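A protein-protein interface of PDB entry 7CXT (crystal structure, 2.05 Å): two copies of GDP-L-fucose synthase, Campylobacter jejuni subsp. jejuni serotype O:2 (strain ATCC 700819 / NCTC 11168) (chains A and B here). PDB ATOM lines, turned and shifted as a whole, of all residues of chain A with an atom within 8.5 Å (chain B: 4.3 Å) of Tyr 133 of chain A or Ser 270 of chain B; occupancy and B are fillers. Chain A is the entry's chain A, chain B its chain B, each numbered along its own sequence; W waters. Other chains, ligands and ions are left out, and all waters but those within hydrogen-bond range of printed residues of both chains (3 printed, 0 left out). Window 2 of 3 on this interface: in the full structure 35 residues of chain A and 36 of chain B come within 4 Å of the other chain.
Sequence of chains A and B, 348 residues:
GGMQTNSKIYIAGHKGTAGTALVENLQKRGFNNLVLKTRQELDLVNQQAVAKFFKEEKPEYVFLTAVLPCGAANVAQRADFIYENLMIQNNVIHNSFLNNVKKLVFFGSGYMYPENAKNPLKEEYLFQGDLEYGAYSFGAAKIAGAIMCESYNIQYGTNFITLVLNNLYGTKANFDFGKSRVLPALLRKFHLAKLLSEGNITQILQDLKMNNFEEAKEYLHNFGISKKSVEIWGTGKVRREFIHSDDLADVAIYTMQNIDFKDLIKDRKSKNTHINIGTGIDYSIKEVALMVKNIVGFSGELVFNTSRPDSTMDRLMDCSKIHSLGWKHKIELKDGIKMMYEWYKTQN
No position is printed for both chains.
Water W2 bridges the side-chain carboxylate of Glu 150 of chain B and the side-chain hydroxyl of Tyr 136 of chain A. Water W1 lies within hydrogen-bond range of OE2 of Glu 150 of chain B (2.7 Å), NH2 of Arg 78 of chain A (3.0 Å) and O of Ser 270 of chain B (3.1 Å). Water W3 lies within hydrogen-bond range of OE2 of Glu 150 of chain B (2.7 Å) and NE of Arg 78 of chain A (3.0 Å).
Tyr 133 of chain A touches just these residues of chain B: Ile 154 and Ser 270. Of chain A, only Tyr 133 (3.0 Å) comes within 4 Å of Ser 270 of chain B. Of the printed residues of chain A, Glu 150 of chain B touches Tyr 136 (3.7 Å). Printed residues of chain B within 4 Å of Tyr 136 of chain A: Glu 150. Lys 269 of chain B touches none of the printed residues of chain A. Leu 131 of chain A touches none of the printed residues of chain B. The nearest printed residue of chain B that does not touch Tyr 133 of chain A is Arg 268 of chain B (4.3 Å). The nearest residue of chain A that does not touch Ser 270 of chain B is Arg 78 of chain A (5.2 Å).
NE of Arg 78 of chain A touches CD1 of Ile 154 of chain B (3.6 Å). Ile 154 of chain B touches Tyr 133 of chain A. CE2 of Tyr 136 of chain A touches OE2 of Glu 150 of chain B (3.7 Å).
Of the 8 printed residues of chain B, 4 touch a printed residue of chain A. Hydrophobic or aromatic side chains of chain A within 4 Å of the printed part of chain B: Tyr 133 and Tyr 136. Among the printed residues, 5 pairs touch across the chains. Among the printed residues, Asp or Glu carboxylates within 4 Å of a Lys or Arg side-chain nitrogen of the other chain: Asp 130 of chain A with Lys 271 of chain B (2.3 Å).
OD2 of Asp 130 of chain A sits close to NZ of Lys 271 of chain B (2.3 Å). OH of Tyr 133 of chain A sits at hydrogen-bond distance from O of Ser 270 of chain B.
The backbone NH (N) of Glu 115 of chain A is in hydrogen-bond range of the backbone carbonyl oxygen (O) of Asp 130 of chain A (2.8 Å). NH1 of Arg 78 of chain A sits at hydrogen-bond distance from O of Tyr 133 of chain A. The backbone carbonyl oxygen (O) of Arg 78 of chain A sits at hydrogen-bond distance from the side-chain hydroxyl (OG) of Ser 137 of chain A (2.7 Å).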
ATOM      1  N   CYS A  70     -27.484  17.586  14.900  1.00  0.00           N
ATOM      2  CA  CYS A  70     -27.221  19.005  15.040  1.00  0.00           C
ATOM      3  C   CYS A  70     -26.338  19.482  13.893  1.00  0.00           C
ATOM      4  O   CYS A  70     -25.261  18.932  13.652  1.00  0.00           O
ATOM      5  CB  CYS A  70     -26.557  19.291  16.385  1.00  0.00           C
ATOM      6  SG  CYS A  70     -26.578  21.030  16.831  1.00  0.00           S
ATOM      7  N   VAL A  75     -29.432  24.866  14.153  1.00  0.00           N
ATOM      8  CA  VAL A  75     -28.929  24.911  15.521  1.00  0.00           C
ATOM      9  C   VAL A  75     -29.955  25.525  16.473  1.00  0.00           C
ATOM     10  O   VAL A  75     -29.903  25.275  17.679  1.00  0.00           O
ATOM     11  CB  VAL A  75     -27.567  25.652  15.557  1.00  0.00           C
ATOM     12  CG1 VAL A  75     -27.716  27.100  15.128  1.00  0.00           C
ATOM     13  CG2 VAL A  75     -26.915  25.555  16.939  1.00  0.00           C
ATOM     14  N   ARG A  78     -32.883  23.799  19.812  1.00  0.00           N
ATOM     15  CA  ARG A  78     -32.209  23.345  21.023  1.00  0.00           C
ATOM     16  C   ARG A  78     -33.046  22.330  21.801  1.00  0.00           C
ATOM     17  O   ARG A  78     -32.526  21.300  22.260  1.00  0.00           O
ATOM     18  CB  ARG A  78     -31.907  24.563  21.893  1.00  0.00           C
ATOM     19  CG  ARG A  78     -30.838  24.369  22.956  1.00  0.00           C
ATOM     20  CD  ARG A  78     -30.438  25.732  23.495  1.00  0.00           C
ATOM     21  NE  ARG A  78     -29.261  25.682  24.361  1.00  0.00           N
ATOM     22  CZ  ARG A  78     -28.011  25.644  23.911  1.00  0.00           C
ATOM     23  NH1 ARG A  78     -27.767  25.611  22.599  1.00  0.00           N
ATOM     24  NH2 ARG A  78     -27.003  25.621  24.768  1.00  0.00           N
ATOM     25  N   PHE A  81     -33.440  18.860  19.852  1.00  0.00           N
ATOM     26  CA  PHE A  81     -32.262  17.996  19.838  1.00  0.00           C
ATOM     27  C   PHE A  81     -32.209  17.108  21.063  1.00  0.00           C
ATOM     28  O   PHE A  81     -31.798  15.942  20.973  1.00  0.00           O
ATOM     29  CB  PHE A  81     -30.966  18.818  19.771  1.00  0.00           C
ATOM     30  CG  PHE A  81     -30.757  19.543  18.477  1.00  0.00           C
ATOM     31  CD1 PHE A  81     -31.074  18.952  17.272  1.00  0.00           C
ATOM     32  CD2 PHE A  81     -30.224  20.829  18.473  1.00  0.00           C
ATOM     33  CE1 PHE A  81     -30.871  19.629  16.082  1.00  0.00           C
ATOM     34  CE2 PHE A  81     -30.021  21.509  17.293  1.00  0.00           C
ATOM     35  CZ  PHE A  81     -30.352  20.909  16.093  1.00  0.00           C
ATOM     36  N   TYR A 111     -19.626  15.473  19.903  1.00  0.00           N
ATOM     37  CA  TYR A 111     -20.197  16.566  20.675  1.00  0.00           C
ATOM     38  C   TYR A 111     -20.477  16.169  22.110  1.00  0.00           C
ATOM     39  O   TYR A 111     -20.783  17.043  22.919  1.00  0.00           O
ATOM     40  CB  TYR A 111     -21.494  17.078  20.033  1.00  0.00           C
ATOM     41  CG  TYR A 111     -21.235  17.827  18.761  1.00  0.00           C
ATOM     42  CD1 TYR A 111     -20.476  18.987  18.771  1.00  0.00           C
ATOM     43  CD2 TYR A 111     -21.752  17.383  17.547  1.00  0.00           C
ATOM     44  CE1 TYR A 111     -20.230  19.688  17.606  1.00  0.00           C
ATOM     45  CE2 TYR A 111     -21.517  18.078  16.376  1.00  0.00           C
ATOM     46  CZ  TYR A 111     -20.746  19.227  16.412  1.00  0.00           C
ATOM     47  OH  TYR A 111     -20.500  19.925  15.254  1.00  0.00           O
ATOM     48  N   GLU A 115     -15.834  20.853  25.326  1.00  0.00           N
ATOM     49  CA  GLU A 115     -15.359  21.691  24.232  1.00  0.00           C
ATOM     50  C   GLU A 115     -13.846  21.864  24.277  1.00  0.00           C
ATOM     51  O   GLU A 115     -13.190  21.907  23.229  1.00  0.00           O
ATOM     52  CB  GLU A 115     -16.036  23.061  24.276  1.00  0.00           C
ATOM     53  CG  GLU A 115     -15.496  24.039  23.221  1.00  0.00           C
ATOM     54  CD  GLU A 115     -16.232  25.384  23.190  1.00  0.00           C
ATOM     55  OE1 GLU A 115     -17.086  25.623  24.065  1.00  0.00           O
ATOM     56  OE2 GLU A 115     -15.957  26.194  22.275  1.00  0.00           O
ATOM     57  N   ASP A 130     -17.394  21.598  30.254  1.00  0.00           N
ATOM     58  CA  ASP A 130     -18.604  21.998  29.540  1.00  0.00           C
ATOM     59  C   ASP A 130     -18.534  21.630  28.056  1.00  0.00           C
ATOM     60  O   ASP A 130     -17.469  21.650  27.437  1.00  0.00           O
ATOM     61  CB  ASP A 130     -18.819  23.509  29.689  1.00  0.00           C
ATOM     62  CG  ASP A 130     -20.204  23.867  30.256  1.00  0.00           C
ATOM     63  OD1 ASP A 130     -21.160  23.082  30.071  1.00  0.00           O
ATOM     64  OD2 ASP A 130     -20.332  24.945  30.880  1.00  0.00           O
ATOM     65  N   LEU A 131     -19.695  21.295  27.493  1.00  0.00           N
ATOM     66  CA  LEU A 131     -19.902  21.028  26.080  1.00  0.00           C
ATOM     67  C   LEU A 131     -19.906  22.327  25.270  1.00  0.00           C
ATOM     68  O   LEU A 131     -20.049  23.424  25.804  1.00  0.00           O
ATOM     69  CB  LEU A 131     -21.224  20.277  25.873  1.00  0.00           C
ATOM     70  CG  LEU A 131     -21.426  19.004  26.711  1.00  0.00           C
ATOM     71  CD1 LEU A 131     -22.786  18.346  26.430  1.00  0.00           C
ATOM     72  CD2 LEU A 131     -20.299  18.002  26.460  1.00  0.00           C
ATOM     73  N   GLU A 132     -19.719  22.192  23.962  1.00  0.00           N
ATOM     74  CA  GLU A 132     -19.832  23.344  23.077  1.00  0.00           C
ATOM     75  C   GLU A 132     -21.261  23.881  23.091  1.00  0.00           C
ATOM     76  O   GLU A 132     -22.233  23.116  23.109  1.00  0.00           O
ATOM     77  CB  GLU A 132     -19.417  22.965  21.654  1.00  0.00           C
ATOM     78  CG  GLU A 132     -19.143  24.149  20.745  1.00  0.00           C
ATOM     79  CD  GLU A 132     -20.411  24.718  20.130  1.00  0.00           C
ATOM     80  OE1 GLU A 132     -21.214  23.934  19.564  1.00  0.00           O
ATOM     81  OE2 GLU A 132     -20.611  25.948  20.230  1.00  0.00           O
ATOM     82  N   TYR A 133     -21.381  25.211  23.065  1.00  0.00           N
ATOM     83  CA  TYR A 133     -22.661  25.836  23.394  1.00  0.00           C
ATOM     84  C   TYR A 133     -23.742  25.457  22.394  1.00  0.00           C
ATOM     85  O   TYR A 133     -24.859  25.100  22.786  1.00  0.00           O
ATOM     86  CB  TYR A 133     -22.526  27.362  23.459  1.00  0.00           C
ATOM     87  CG  TYR A 133     -23.844  28.002  23.862  1.00  0.00           C
ATOM     88  CD1 TYR A 133     -24.181  28.129  25.193  1.00  0.00           C
ATOM     89  CD2 TYR A 133     -24.767  28.429  22.911  1.00  0.00           C
ATOM     90  CE1 TYR A 133     -25.385  28.653  25.577  1.00  0.00           C
ATOM     91  CE2 TYR A 133     -26.000  28.999  23.307  1.00  0.00           C
ATOM     92  CZ  TYR A 133     -26.279  29.113  24.650  1.00  0.00           C
ATOM     93  OH  TYR A 133     -27.465  29.648  25.094  1.00  0.00           O
ATOM     94  N   GLY A 134     -23.421  25.490  21.097  1.00  0.00           N
ATOM     95  CA  GLY A 134     -24.427  25.200  20.088  1.00  0.00           C
ATOM     96  C   GLY A 134     -24.892  23.759  20.109  1.00  0.00           C
ATOM     97  O   GLY A 134     -26.067  23.475  19.856  1.00  0.00           O
ATOM     98  N   ALA A 135     -24.003  22.838  20.451  1.00  0.00           N
ATOM     99  CA  ALA A 135     -24.325  21.423  20.508  1.00  0.00           C
ATOM    100  C   ALA A 135     -24.602  20.956  21.928  1.00  0.00           C
ATOM    101  O   ALA A 135     -24.642  19.750  22.178  1.00  0.00           O
ATOM    102  CB  ALA A 135     -23.192  20.610  19.888  1.00  0.00           C
ATOM    103  N   TYR A 136     -24.804  21.893  22.852  1.00  0.00           N
ATOM    104  CA  TYR A 136     -24.920  21.568  24.273  1.00  0.00           C
ATOM    105  C   TYR A 136     -26.042  20.564  24.560  1.00  0.00           C
ATOM    106  O   TYR A 136     -25.838  19.576  25.274  1.00  0.00           O
ATOM    107  CB  TYR A 136     -25.145  22.872  25.036  1.00  0.00           C
ATOM    108  CG  TYR A 136     -25.305  22.791  26.533  1.00  0.00           C
ATOM    109  CD1 TYR A 136     -24.195  22.682  27.366  1.00  0.00           C
ATOM    110  CD2 TYR A 136     -26.558  22.919  27.118  1.00  0.00           C
ATOM    111  CE1 TYR A 136     -24.339  22.652  28.755  1.00  0.00           C
ATOM    112  CE2 TYR A 136     -26.712  22.895  28.496  1.00  0.00           C
ATOM    113  CZ  TYR A 136     -25.602  22.766  29.309  1.00  0.00           C
ATOM    114  OH  TYR A 136     -25.770  22.753  30.674  1.00  0.00           O
ATOM    115  N   SER A 137     -27.246  20.815  24.057  1.00  0.00           N
ATOM    116  CA  SER A 137     -28.335  19.899  24.385  1.00  0.00           C
ATOM    117  C   SER A 137     -28.256  18.613  23.566  1.00  0.00           C
ATOM    118  O   SER A 137     -28.655  17.544  24.050  1.00  0.00           O
ATOM    119  CB  SER A 137     -29.692  20.591  24.187  1.00  0.00           C
ATOM    120  OG  SER A 137     -29.908  20.934  22.832  1.00  0.00           O
ATOM    121  N   PHE A 138     -27.744  18.700  22.337  1.00  0.00           N
ATOM    122  CA  PHE A 138     -27.508  17.502  21.533  1.00  0.00           C
ATOM    123  C   PHE A 138     -26.468  16.610  22.188  1.00  0.00           C
ATOM    124  O   PHE A 138     -26.656  15.393  22.282  1.00  0.00           O
ATOM    125  CB  PHE A 138     -27.061  17.898  20.124  1.00  0.00           C
ATOM    126  CG  PHE A 138     -26.743  16.724  19.221  1.00  0.00           C
ATOM    127  CD1 PHE A 138     -27.756  16.034  18.570  1.00  0.00           C
ATOM    128  CD2 PHE A 138     -25.414  16.329  19.006  1.00  0.00           C
ATOM    129  CE1 PHE A 138     -27.462  14.954  17.722  1.00  0.00           C
ATOM    130  CE2 PHE A 138     -25.109  15.245  18.181  1.00  0.00           C
ATOM    131  CZ  PHE A 138     -26.136  14.550  17.541  1.00  0.00           C
ATOM    132  N   GLY A 139     -25.388  17.203  22.698  1.00  0.00           N
ATOM    133  CA  GLY A 139     -24.358  16.398  23.326  1.00  0.00           C
ATOM    134  C   GLY A 139     -24.834  15.767  24.614  1.00  0.00           C
ATOM    135  O   GLY A 139     -24.553  14.596  24.879  1.00  0.00           O
ATOM    136  N   MET A 313     -14.017  24.175  17.772  1.00  0.00           N
ATOM    137  CA  MET A 313     -12.992  23.358  18.404  1.00  0.00           C
ATOM    138  C   MET A 313     -12.521  22.261  17.451  1.00  0.00           C
ATOM    139  O   MET A 313     -13.240  21.851  16.546  1.00  0.00           O
ATOM    140  CB  MET A 313     -13.556  22.727  19.684  1.00  0.00           C
ATOM    141  CG  MET A 313     -14.555  21.601  19.411  1.00  0.00           C
ATOM    142  SD  MET A 313     -15.971  21.429  20.524  1.00  0.00           S
ATOM    143  CE  MET A 313     -17.231  20.994  19.318  1.00  0.00           C
ATOM    144  N   GLU B 150     -34.303  24.169  30.301  1.00  0.00           N
ATOM    145  CA  GLU B 150     -33.669  25.367  29.767  1.00  0.00           C
ATOM    146  C   GLU B 150     -33.775  25.417  28.247  1.00  0.00           C
ATOM    147  O   GLU B 150     -34.001  26.488  27.670  1.00  0.00           O
ATOM    148  CB  GLU B 150     -32.207  25.413  30.213  1.00  0.00           C
ATOM    149  CG  GLU B 150     -31.401  26.480  29.532  1.00  0.00           C
ATOM    150  CD  GLU B 150     -29.941  26.412  29.940  1.00  0.00           C
ATOM    151  OE1 GLU B 150     -29.554  27.179  30.842  1.00  0.00           O
ATOM    152  OE2 GLU B 150     -29.194  25.561  29.385  1.00  0.00           O
ATOM    153  N   ILE B 154     -35.403  28.220  25.867  1.00  0.00           N
ATOM    154  CA  ILE B 154     -34.646  28.996  24.887  1.00  0.00           C
ATOM    155  C   ILE B 154     -35.308  28.936  23.522  1.00  0.00           C
ATOM    156  O   ILE B 154     -35.535  29.969  22.884  1.00  0.00           O
ATOM    157  CB  ILE B 154     -33.183  28.511  24.802  1.00  0.00           C
ATOM    158  CG1 ILE B 154     -32.406  28.910  26.052  1.00  0.00           C
ATOM    159  CG2 ILE B 154     -32.485  29.052  23.518  1.00  0.00           C
ATOM    160  CD1 ILE B 154     -30.980  28.347  26.081  1.00  0.00           C
ATOM    161  N   ILE B 265     -31.524  34.906  32.887  1.00  0.00           N
ATOM    162  CA  ILE B 265     -30.579  34.860  31.781  1.00  0.00           C
ATOM    163  C   ILE B 265     -29.743  36.132  31.786  1.00  0.00           C
ATOM    164  O   ILE B 265     -30.285  37.245  31.797  1.00  0.00           O
ATOM    165  CB  ILE B 265     -31.294  34.649  30.442  1.00  0.00           C
ATOM    166  CG1 ILE B 265     -32.472  35.611  30.294  1.00  0.00           C
ATOM    167  CG2 ILE B 265     -31.794  33.217  30.365  1.00  0.00           C
ATOM    168  CD1 ILE B 265     -33.314  35.314  29.084  1.00  0.00           C
ATOM    169  N   ASP B 267     -28.113  37.832  29.465  1.00  0.00           N
ATOM    170  CA  ASP B 267     -28.099  38.051  28.019  1.00  0.00           C
ATOM    171  C   ASP B 267     -27.657  36.825  27.231  1.00  0.00           C
ATOM    172  O   ASP B 267     -28.282  35.760  27.300  1.00  0.00           O
ATOM    173  CB  ASP B 267     -27.188  39.225  27.638  1.00  0.00           C
ATOM    174  CG  ASP B 267     -26.689  40.005  28.836  1.00  0.00           C
ATOM    175  OD1 ASP B 267     -27.511  40.371  29.702  1.00  0.00           O
ATOM    176  OD2 ASP B 267     -25.465  40.248  28.908  1.00  0.00           O
ATOM    177  N   ARG B 268     -26.557  36.979  26.488  1.00  0.00           N
ATOM    178  CA  ARG B 268     -26.051  35.895  25.651  1.00  0.00           C
ATOM    179  C   ARG B 268     -25.653  34.673  26.475  1.00  0.00           C
ATOM    180  O   ARG B 268     -25.763  33.541  25.989  1.00  0.00           O
ATOM    181  CB  ARG B 268     -24.879  36.419  24.811  1.00  0.00           C
ATOM    182  CG  ARG B 268     -24.012  35.358  24.145  1.00  0.00           C
ATOM    183  CD  ARG B 268     -22.685  35.197  24.877  1.00  0.00           C
ATOM    184  NE  ARG B 268     -22.162  36.477  25.349  1.00  0.00           N
ATOM    185  CZ  ARG B 268     -21.414  37.299  24.619  1.00  0.00           C
ATOM    186  NH1 ARG B 268     -21.095  36.981  23.371  1.00  0.00           N
ATOM    187  NH2 ARG B 268     -20.987  38.444  25.137  1.00  0.00           N
ATOM    188  N   LYS B 269     -25.239  34.860  27.728  1.00  0.00           N
ATOM    189  CA  LYS B 269     -24.805  33.728  28.553  1.00  0.00           C
ATOM    190  C   LYS B 269     -26.013  33.142  29.285  1.00  0.00           C
ATOM    191  O   LYS B 269     -26.165  33.276  30.501  1.00  0.00           O
ATOM    192  CB  LYS B 269     -23.713  34.164  29.526  1.00  0.00           C
ATOM    193  CG  LYS B 269     -22.743  33.064  29.856  1.00  0.00           C
ATOM    194  CD  LYS B 269     -21.590  33.530  30.753  1.00  0.00           C
ATOM    195  CE  LYS B 269     -20.530  32.422  30.901  1.00  0.00           C
ATOM    196  NZ  LYS B 269     -21.081  31.153  31.452  1.00  0.00           N
ATOM    197  N   SER B 270     -26.893  32.518  28.504  1.00  0.00           N
ATOM    198  CA  SER B 270     -28.001  31.715  29.042  1.00  0.00           C
ATOM    199  C   SER B 270     -27.539  30.262  29.077  1.00  0.00           C
ATOM    200  O   SER B 270     -27.621  29.522  28.090  1.00  0.00           O
ATOM    201  CB  SER B 270     -29.275  31.887  28.228  1.00  0.00           C
ATOM    202  OG  SER B 270     -29.041  31.767  26.839  1.00  0.00           O
ATOM    203  N   LYS B 271     -27.002  29.877  30.227  1.00  0.00           N
ATOM    204  CA  LYS B 271     -26.745  28.492  30.587  1.00  0.00           C
ATOM    205  C   LYS B 271     -26.677  28.489  32.097  1.00  0.00           C
ATOM    206  O   LYS B 271     -26.568  29.550  32.718  1.00  0.00           O
ATOM    207  CB  LYS B 271     -25.471  27.927  29.947  1.00  0.00           C
ATOM    208  CG  LYS B 271     -24.157  28.444  30.457  1.00  0.00           C
ATOM    209  CD  LYS B 271     -23.024  27.557  29.890  1.00  0.00           C
ATOM    210  CE  LYS B 271     -21.645  28.035  30.301  1.00  0.00           C
ATOM    211  NZ  LYS B 271     -20.573  27.065  29.908  1.00  0.00           N
HETATM  212  O   HOH W   1     -27.401  26.457  27.640  1.00  0.00           O
HETATM  213  O   HOH W   2     -27.578  24.938  31.336  1.00  0.00           O
HETATM  214  O   HOH W   3     -30.074  24.650  27.009  1.00  0.00           O
